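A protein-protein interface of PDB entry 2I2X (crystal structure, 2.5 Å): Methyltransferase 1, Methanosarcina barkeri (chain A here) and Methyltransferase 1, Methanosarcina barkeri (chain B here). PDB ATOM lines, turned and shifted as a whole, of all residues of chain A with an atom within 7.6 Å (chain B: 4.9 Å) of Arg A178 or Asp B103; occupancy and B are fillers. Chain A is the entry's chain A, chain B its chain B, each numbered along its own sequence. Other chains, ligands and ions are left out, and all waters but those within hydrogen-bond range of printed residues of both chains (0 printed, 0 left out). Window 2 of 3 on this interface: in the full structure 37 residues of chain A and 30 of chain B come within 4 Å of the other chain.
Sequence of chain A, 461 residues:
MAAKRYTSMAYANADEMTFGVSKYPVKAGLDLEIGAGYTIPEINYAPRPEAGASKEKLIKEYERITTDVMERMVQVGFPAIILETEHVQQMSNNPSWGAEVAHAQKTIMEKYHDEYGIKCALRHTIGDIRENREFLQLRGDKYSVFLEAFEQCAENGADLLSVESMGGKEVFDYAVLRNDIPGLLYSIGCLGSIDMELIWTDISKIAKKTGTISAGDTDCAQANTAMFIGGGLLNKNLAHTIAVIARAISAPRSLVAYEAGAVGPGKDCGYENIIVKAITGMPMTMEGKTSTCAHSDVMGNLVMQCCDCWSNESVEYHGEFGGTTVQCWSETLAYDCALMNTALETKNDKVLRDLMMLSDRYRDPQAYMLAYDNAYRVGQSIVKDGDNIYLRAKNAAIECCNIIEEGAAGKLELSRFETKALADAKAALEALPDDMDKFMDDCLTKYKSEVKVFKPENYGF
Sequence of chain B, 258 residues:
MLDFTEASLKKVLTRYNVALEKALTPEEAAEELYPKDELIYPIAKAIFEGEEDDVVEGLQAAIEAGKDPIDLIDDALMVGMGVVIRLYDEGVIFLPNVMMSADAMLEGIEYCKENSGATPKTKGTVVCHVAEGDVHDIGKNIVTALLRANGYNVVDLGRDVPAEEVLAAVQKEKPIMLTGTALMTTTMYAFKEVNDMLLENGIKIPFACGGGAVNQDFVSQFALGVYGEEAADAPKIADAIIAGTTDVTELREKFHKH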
ATOM      1  N   VAL A 171     -19.567   1.556  26.171  1.00  0.00           N
ATOM      2  CA  VAL A 171     -18.523   0.784  25.508  1.00  0.00           C
ATOM      3  C   VAL A 171     -17.709   1.637  24.540  1.00  0.00           C
ATOM      4  O   VAL A 171     -16.497   1.426  24.401  1.00  0.00           O
ATOM      5  CB  VAL A 171     -19.068  -0.499  24.823  1.00  0.00           C
ATOM      6  CG1 VAL A 171     -17.931  -1.269  24.156  1.00  0.00           C
ATOM      7  CG2 VAL A 171     -19.761  -1.372  25.846  1.00  0.00           C
ATOM      8  N   PHE A 172     -18.366   2.599  23.885  1.00  0.00           N
ATOM      9  CA  PHE A 172     -17.666   3.578  23.044  1.00  0.00           C
ATOM     10  C   PHE A 172     -16.604   4.360  23.828  1.00  0.00           C
ATOM     11  O   PHE A 172     -15.464   4.508  23.363  1.00  0.00           O
ATOM     12  CB  PHE A 172     -18.632   4.569  22.354  1.00  0.00           C
ATOM     13  CG  PHE A 172     -17.925   5.776  21.784  1.00  0.00           C
ATOM     14  CD1 PHE A 172     -17.410   5.743  20.492  1.00  0.00           C
ATOM     15  CD2 PHE A 172     -17.692   6.902  22.578  1.00  0.00           C
ATOM     16  CE1 PHE A 172     -16.716   6.799  19.976  1.00  0.00           C
ATOM     17  CE2 PHE A 172     -16.975   7.978  22.073  1.00  0.00           C
ATOM     18  CZ  PHE A 172     -16.492   7.924  20.762  1.00  0.00           C
ATOM     19  N   ASP A 173     -16.978   4.876  24.999  1.00  0.00           N
ATOM     20  CA  ASP A 173     -16.063   5.699  25.804  1.00  0.00           C
ATOM     21  C   ASP A 173     -14.797   4.960  26.188  1.00  0.00           C
ATOM     22  O   ASP A 173     -13.705   5.550  26.195  1.00  0.00           O
ATOM     23  CB  ASP A 173     -16.743   6.182  27.068  1.00  0.00           C
ATOM     24  CG  ASP A 173     -17.694   7.337  26.822  1.00  0.00           C
ATOM     25  OD1 ASP A 173     -17.574   8.060  25.797  1.00  0.00           O
ATOM     26  OD2 ASP A 173     -18.573   7.528  27.688  1.00  0.00           O
ATOM     27  N   TYR A 174     -14.966   3.676  26.540  1.00  0.00           N
ATOM     28  CA  TYR A 174     -13.867   2.756  26.765  1.00  0.00           C
ATOM     29  C   TYR A 174     -13.063   2.514  25.482  1.00  0.00           C
ATOM     30  O   TYR A 174     -11.855   2.725  25.476  1.00  0.00           O
ATOM     31  CB  TYR A 174     -14.383   1.433  27.380  1.00  0.00           C
ATOM     32  CG  TYR A 174     -13.333   0.348  27.518  1.00  0.00           C
ATOM     33  CD1 TYR A 174     -13.201  -0.633  26.531  1.00  0.00           C
ATOM     34  CD2 TYR A 174     -12.459   0.313  28.625  1.00  0.00           C
ATOM     35  CE1 TYR A 174     -12.236  -1.633  26.634  1.00  0.00           C
ATOM     36  CE2 TYR A 174     -11.482  -0.699  28.754  1.00  0.00           C
ATOM     37  CZ  TYR A 174     -11.380  -1.672  27.745  1.00  0.00           C
ATOM     38  OH  TYR A 174     -10.441  -2.698  27.808  1.00  0.00           O
ATOM     39  N   ALA A 175     -13.725   2.086  24.403  1.00  0.00           N
ATOM     40  CA  ALA A 175     -13.059   1.800  23.120  1.00  0.00           C
ATOM     41  C   ALA A 175     -12.294   2.983  22.496  1.00  0.00           C
ATOM     42  O   ALA A 175     -11.184   2.795  21.977  1.00  0.00           O
ATOM     43  CB  ALA A 175     -14.057   1.251  22.125  1.00  0.00           C
ATOM     44  N   VAL A 176     -12.885   4.187  22.532  1.00  0.00           N
ATOM     45  CA  VAL A 176     -12.272   5.332  21.857  1.00  0.00           C
ATOM     46  C   VAL A 176     -10.940   5.785  22.470  1.00  0.00           C
ATOM     47  O   VAL A 176     -10.116   6.374  21.793  1.00  0.00           O
ATOM     48  CB  VAL A 176     -13.260   6.528  21.672  1.00  0.00           C
ATOM     49  CG1 VAL A 176     -13.394   7.372  22.929  1.00  0.00           C
ATOM     50  CG2 VAL A 176     -12.838   7.346  20.487  1.00  0.00           C
ATOM     51  N   LEU A 177     -10.735   5.507  23.750  1.00  0.00           N
ATOM     52  CA  LEU A 177      -9.460   5.835  24.389  1.00  0.00           C
ATOM     53  C   LEU A 177      -8.369   4.805  24.067  1.00  0.00           C
ATOM     54  O   LEU A 177      -7.231   4.981  24.478  1.00  0.00           O
ATOM     55  CB  LEU A 177      -9.640   5.962  25.905  1.00  0.00           C
ATOM     56  CG  LEU A 177     -10.008   7.305  26.563  1.00  0.00           C
ATOM     57  CD1 LEU A 177     -10.297   8.448  25.597  1.00  0.00           C
ATOM     58  CD2 LEU A 177     -11.146   7.152  27.550  1.00  0.00           C
ATOM     59  N   ARG A 178      -8.708   3.751  23.317  1.00  0.00           N
ATOM     60  CA  ARG A 178      -7.811   2.602  23.170  1.00  0.00           C
ATOM     61  C   ARG A 178      -7.574   2.123  21.763  1.00  0.00           C
ATOM     62  O   ARG A 178      -6.983   1.061  21.575  1.00  0.00           O
ATOM     63  CB  ARG A 178      -8.293   1.426  24.047  1.00  0.00           C
ATOM     64  CG  ARG A 178      -8.394   1.824  25.516  1.00  0.00           C
ATOM     65  CD  ARG A 178      -8.983   0.796  26.480  1.00  0.00           C
ATOM     66  NE  ARG A 178      -8.667   1.266  27.841  1.00  0.00           N
ATOM     67  CZ  ARG A 178      -9.320   2.234  28.489  1.00  0.00           C
ATOM     68  NH1 ARG A 178     -10.390   2.830  27.956  1.00  0.00           N
ATOM     69  NH2 ARG A 178      -8.912   2.599  29.688  1.00  0.00           N
ATOM     70  N   ASN A 179      -7.993   2.889  20.760  1.00  0.00           N
ATOM     71  CA  ASN A 179      -7.878   2.436  19.365  1.00  0.00           C
ATOM     72  C   ASN A 179      -8.499   1.049  19.178  1.00  0.00           C
ATOM     73  O   ASN A 179      -8.041   0.242  18.365  1.00  0.00           O
ATOM     74  CB  ASN A 179      -6.426   2.475  18.889  1.00  0.00           C
ATOM     75  CG  ASN A 179      -5.875   3.916  18.791  1.00  0.00           C
ATOM     76  OD1 ASN A 179      -6.633   4.893  18.744  1.00  0.00           O
ATOM     77  ND2 ASN A 179      -4.555   4.042  18.767  1.00  0.00           N
ATOM     78  N   ASP A 180      -9.545   0.785  19.954  1.00  0.00           N
ATOM     79  CA  ASP A 180     -10.262  -0.467  19.855  1.00  0.00           C
ATOM     80  C   ASP A 180     -11.328  -0.307  18.765  1.00  0.00           C
ATOM     81  O   ASP A 180     -12.500   0.036  19.028  1.00  0.00           O
ATOM     82  CB  ASP A 180     -10.844  -0.874  21.218  1.00  0.00           C
ATOM     83  CG  ASP A 180     -11.520  -2.235  21.182  1.00  0.00           C
ATOM     84  OD1 ASP A 180     -11.635  -2.837  20.078  1.00  0.00           O
ATOM     85  OD2 ASP A 180     -11.936  -2.714  22.266  1.00  0.00           O
ATOM     86  N   ILE A 181     -10.899  -0.529  17.527  1.00  0.00           N
ATOM     87  CA  ILE A 181     -11.777  -0.389  16.378  1.00  0.00           C
ATOM     88  C   ILE A 181     -13.013  -1.323  16.404  1.00  0.00           C
ATOM     89  O   ILE A 181     -14.153  -0.850  16.224  1.00  0.00           O
ATOM     90  CB  ILE A 181     -11.011  -0.566  15.092  1.00  0.00           C
ATOM     91  CG1 ILE A 181      -9.803   0.376  15.057  1.00  0.00           C
ATOM     92  CG2 ILE A 181     -11.935  -0.358  13.931  1.00  0.00           C
ATOM     93  CD1 ILE A 181     -10.068   1.840  15.473  1.00  0.00           C
ATOM     94  N   LEU A 184     -15.445   0.094  18.708  1.00  0.00           N
ATOM     95  CA  LEU A 184     -16.183   1.114  17.975  1.00  0.00           C
ATOM     96  C   LEU A 184     -17.334   0.515  17.170  1.00  0.00           C
ATOM     97  O   LEU A 184     -18.472   0.981  17.296  1.00  0.00           O
ATOM     98  CB  LEU A 184     -15.242   1.922  17.072  1.00  0.00           C
ATOM     99  CG  LEU A 184     -14.551   3.226  17.514  1.00  0.00           C
ATOM    100  CD1 LEU A 184     -14.551   3.526  19.013  1.00  0.00           C
ATOM    101  CD2 LEU A 184     -13.124   3.259  16.946  1.00  0.00           C
ATOM    102  N   ASN A 237      -4.623  13.650  20.447  1.00  0.00           N
ATOM    103  CA  ASN A 237      -5.462  12.820  21.295  1.00  0.00           C
ATOM    104  C   ASN A 237      -6.206  11.660  20.620  1.00  0.00           C
ATOM    105  O   ASN A 237      -6.605  10.707  21.288  1.00  0.00           O
ATOM    106  CB  ASN A 237      -6.379  13.679  22.158  1.00  0.00           C
ATOM    107  CG  ASN A 237      -5.607  14.465  23.231  1.00  0.00           C
ATOM    108  OD1 ASN A 237      -4.540  14.032  23.712  1.00  0.00           O
ATOM    109  ND2 ASN A 237      -6.133  15.629  23.599  1.00  0.00           N
ATOM    110  N   LEU A 238      -6.377  11.738  19.299  1.00  0.00           N
ATOM    111  CA  LEU A 238      -7.050  10.688  18.534  1.00  0.00           C
ATOM    112  C   LEU A 238      -6.779  10.948  17.056  1.00  0.00           C
ATOM    113  O   LEU A 238      -7.070  12.045  16.545  1.00  0.00           O
ATOM    114  CB  LEU A 238      -8.567  10.676  18.784  1.00  0.00           C
ATOM    115  CG  LEU A 238      -9.294   9.557  18.025  1.00  0.00           C
ATOM    116  CD1 LEU A 238      -8.985   8.132  18.610  1.00  0.00           C
ATOM    117  CD2 LEU A 238     -10.798   9.796  17.993  1.00  0.00           C
ATOM    118  N   ILE A 242      -9.041   7.677  12.631  1.00  0.00           N
ATOM    119  CA  ILE A 242      -9.927   6.841  13.452  1.00  0.00           C
ATOM    120  C   ILE A 242     -11.270   7.550  13.735  1.00  0.00           C
ATOM    121  O   ILE A 242     -12.338   6.908  13.851  1.00  0.00           O
ATOM    122  CB  ILE A 242      -9.230   6.346  14.777  1.00  0.00           C
ATOM    123  CG1 ILE A 242      -8.092   5.358  14.460  1.00  0.00           C
ATOM    124  CG2 ILE A 242     -10.226   5.656  15.694  1.00  0.00           C
ATOM    125  CD1 ILE A 242      -7.087   5.196  15.600  1.00  0.00           C
ATOM    126  N   GLU A 450     -14.176  -6.519  30.296  1.00  0.00           N
ATOM    127  CA  GLU A 450     -13.350  -5.294  30.255  1.00  0.00           C
ATOM    128  C   GLU A 450     -13.995  -4.010  30.755  1.00  0.00           C
ATOM    129  O   GLU A 450     -13.287  -3.106  31.172  1.00  0.00           O
ATOM    130  CB  GLU A 450     -12.747  -5.074  28.873  1.00  0.00           C
ATOM    131  CG  GLU A 450     -11.855  -6.235  28.436  1.00  0.00           C
ATOM    132  CD  GLU A 450     -11.031  -5.923  27.210  1.00  0.00           C
ATOM    133  OE1 GLU A 450     -11.011  -4.744  26.751  1.00  0.00           O
ATOM    134  OE2 GLU A 450     -10.393  -6.870  26.700  1.00  0.00           O
ATOM    135  N   VAL A 451     -15.322  -3.929  30.730  1.00  0.00           N
ATOM    136  CA  VAL A 451     -16.003  -2.676  31.038  1.00  0.00           C
ATOM    137  C   VAL A 451     -17.039  -2.885  32.116  1.00  0.00           C
ATOM    138  O   VAL A 451     -18.158  -3.282  31.818  1.00  0.00           O
ATOM    139  CB  VAL A 451     -16.734  -2.132  29.799  1.00  0.00           C
ATOM    140  CG1 VAL A 451     -17.307  -0.719  30.076  1.00  0.00           C
ATOM    141  CG2 VAL A 451     -15.829  -2.150  28.588  1.00  0.00           C
ATOM    142  N   PRO B  96      -4.368   7.618  22.916  1.00  0.00           N
ATOM    143  CA  PRO B  96      -4.714   6.212  23.097  1.00  0.00           C
ATOM    144  C   PRO B  96      -3.515   5.301  23.279  1.00  0.00           C
ATOM    145  O   PRO B  96      -3.654   4.215  23.831  1.00  0.00           O
ATOM    146  CB  PRO B  96      -5.514   5.876  21.828  1.00  0.00           C
ATOM    147  CG  PRO B  96      -6.115   7.189  21.447  1.00  0.00           C
ATOM    148  CD  PRO B  96      -4.961   8.139  21.670  1.00  0.00           C
ATOM    149  N   MET B  99      -2.879   5.490  26.981  1.00  0.00           N
ATOM    150  CA  MET B  99      -3.885   4.725  27.718  1.00  0.00           C
ATOM    151  C   MET B  99      -3.613   3.213  27.752  1.00  0.00           C
ATOM    152  O   MET B  99      -3.718   2.592  28.802  1.00  0.00           O
ATOM    153  CB  MET B  99      -5.292   4.976  27.167  1.00  0.00           C
ATOM    154  CG  MET B  99      -5.822   6.368  27.363  1.00  0.00           C
ATOM    155  SD  MET B  99      -5.737   6.887  29.070  1.00  0.00           S
ATOM    156  CE  MET B  99      -7.382   6.516  29.670  1.00  0.00           C
ATOM    157  N   MET B 100      -3.277   2.643  26.598  1.00  0.00           N
ATOM    158  CA  MET B 100      -2.993   1.231  26.460  1.00  0.00           C
ATOM    159  C   MET B 100      -1.758   0.852  27.261  1.00  0.00           C
ATOM    160  O   MET B 100      -1.706  -0.223  27.856  1.00  0.00           O
ATOM    161  CB  MET B 100      -2.765   0.882  25.000  1.00  0.00           C
ATOM    162  CG  MET B 100      -4.013   0.529  24.238  1.00  0.00           C
ATOM    163  SD  MET B 100      -3.693   0.625  22.464  1.00  0.00           S
ATOM    164  CE  MET B 100      -2.404  -0.611  22.230  1.00  0.00           C
ATOM    165  N   SER B 101      -0.778   1.748  27.271  1.00  0.00           N
ATOM    166  CA  SER B 101       0.432   1.585  28.051  1.00  0.00           C
ATOM    167  C   SER B 101       0.144   1.639  29.549  1.00  0.00           C
ATOM    168  O   SER B 101       0.761   0.904  30.328  1.00  0.00           O
ATOM    169  CB  SER B 101       1.467   2.650  27.656  1.00  0.00           C
ATOM    170  OG  SER B 101       1.986   2.398  26.357  1.00  0.00           O
ATOM    171  N   ALA B 102      -0.789   2.501  29.945  1.00  0.00           N
ATOM    172  CA  ALA B 102      -1.172   2.638  31.347  1.00  0.00           C
ATOM    173  C   ALA B 102      -1.951   1.410  31.818  1.00  0.00           C
ATOM    174  O   ALA B 102      -1.798   0.981  32.958  1.00  0.00           O
ATOM    175  CB  ALA B 102      -1.983   3.905  31.562  1.00  0.00           C
ATOM    176  N   ASP B 103      -2.790   0.864  30.933  1.00  0.00           N
ATOM    177  CA  ASP B 103      -3.456  -0.423  31.150  1.00  0.00           C
ATOM    178  C   ASP B 103      -2.417  -1.517  31.359  1.00  0.00           C
ATOM    179  O   ASP B 103      -2.495  -2.285  32.313  1.00  0.00           O
ATOM    180  CB  ASP B 103      -4.317  -0.795  29.944  1.00  0.00           C
ATOM    181  CG  ASP B 103      -5.623  -0.047  29.904  1.00  0.00           C
ATOM    182  OD1 ASP B 103      -5.931   0.693  30.862  1.00  0.00           O
ATOM    183  OD2 ASP B 103      -6.347  -0.210  28.897  1.00  0.00           O
ATOM    184  N   ALA B 104      -1.450  -1.579  30.451  1.00  0.00           N
ATOM    185  CA  ALA B 104      -0.391  -2.572  30.508  1.00  0.00           C
ATOM    186  C   ALA B 104       0.457  -2.427  31.771  1.00  0.00           C
ATOM    187  O   ALA B 104       0.823  -3.422  32.386  1.00  0.00           O
ATOM    188  CB  ALA B 104       0.478  -2.489  29.268  1.00  0.00           C
ATOM    189  N   MET B 105       0.740  -1.185  32.162  1.00  0.00           N
ATOM    190  CA  MET B 105       1.570  -0.912  33.334  1.00  0.00           C
ATOM    191  C   MET B 105       0.843  -1.178  34.646  1.00  0.00           C
ATOM    192  O   MET B 105       1.423  -1.749  35.565  1.00  0.00           O
ATOM    193  CB  MET B 105       2.071   0.525  33.311  1.00  0.00           C
ATOM    194  CG  MET B 105       2.885   0.918  34.525  1.00  0.00           C
ATOM    195  SD  MET B 105       2.508   2.598  35.055  1.00  0.00           S
ATOM    196  CE  MET B 105       0.759   2.464  35.460  1.00  0.00           C
ATOM    197  N   LEU B 106      -0.413  -0.746  34.738  1.00  0.00           N
ATOM    198  CA  LEU B 106      -1.242  -1.019  35.912  1.00  0.00           C
ATOM    199  C   LEU B 106      -1.408  -2.521  36.170  1.00  0.00           C
ATOM    200  O   LEU B 106      -1.487  -2.951  37.325  1.00  0.00           O
ATOM    201  CB  LEU B 106      -2.621  -0.368  35.769  1.00  0.00           C
ATOM    202  CG  LEU B 106      -2.785   1.099  36.168  1.00  0.00           C
ATOM    203  CD1 LEU B 106      -3.955   1.724  35.409  1.00  0.00           C
ATOM    204  CD2 LEU B 106      -2.978   1.238  37.676  1.00  0.00           C
ATOM    205  N   GLU B 107      -1.465  -3.306  35.092  1.00  0.00           N
ATOM    206  CA  GLU B 107      -1.601  -4.755  35.190  1.00  0.00           C
ATOM    207  C   GLU B 107      -0.261  -5.395  35.552  1.00  0.00           C
ATOM    208  O   GLU B 107      -0.190  -6.583  35.898  1.00  0.00           O
ATOM    209  CB  GLU B 107      -2.138  -5.335  33.887  1.00  0.00           C
ATOM    210  CG  GLU B 107      -3.144  -6.450  34.109  1.00  0.00           C
ATOM    211  CD  GLU B 107      -3.374  -7.282  32.869  1.00  0.00           C
ATOM    212  OE1 GLU B 107      -4.546  -7.415  32.453  1.00  0.00           O
ATOM    213  OE2 GLU B 107      -2.381  -7.796  32.309  1.00  0.00           O
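NE of Arg A178 is in salt-bridge range of OD2 of Asp B103, 2.9 Å away.
The side-chain sulfur (SD) of Met B100 lies close to the backbone carbonyl oxygen (O) of Arg A178 (3.4 Å).
O of Tyr A174 is in hydrogen-bond range of NH1 of Arg A178 (2.9 Å).
Among the printed residues, merely in contact across the chains: Asn A237 with Pro B96 (3.1 Å), Leu A177 with Pro B96 (3.1 Å), Leu A177 with Met B99 (3.3 Å) and Asn A179 with Pro B96 (3.4 Å).
Arg A178 touches just these residues of chain B: Met B100 (3.4 Å) and Asp B103 (2.9 Å).
Asp B103 touches just one residue of chain A: Arg A178 (2.9 Å).
Ala B102 touches none of the printed residues of chain A.
Printed residues of chain B within 4 Å of Leu A177: Pro B96 and Met B99.
Of the printed residues of chain B, Asn A237 touches Pro B96 (3.1 Å).
Printed residues of chain A within 4 Å of Pro B96: Leu A177, Asn A179 and Asn A237.
Printed residues of chain A within 4 Å of Met B99: Leu A177.
The nearest residue of chain B that does not touch Arg A178 is Pro B96 (4.1 Å).
The nearest printed residue of chain B that does not touch Leu A177 is Met B100 (5.1 Å).
Of the 10 printed residues of chain B, 4 touch a printed residue of chain A.
Printed residues of chain B that touch a printed residue of chain A: Pro B96, Met B99, Met B100 and Asp B103.
Hydrophobic or aromatic side chains of chain B that line the printed part of chain A: Pro B96, Met B99 and Met B100.
Of the 17 printed residues of chain A, 4 touch a printed residue of chain B.
Among the printed residues, Asp or Glu carboxylates within 4 Å of a Lys or Arg side-chain nitrogen of the other chain: Arg A178 with Asp B103 (2.9 Å).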
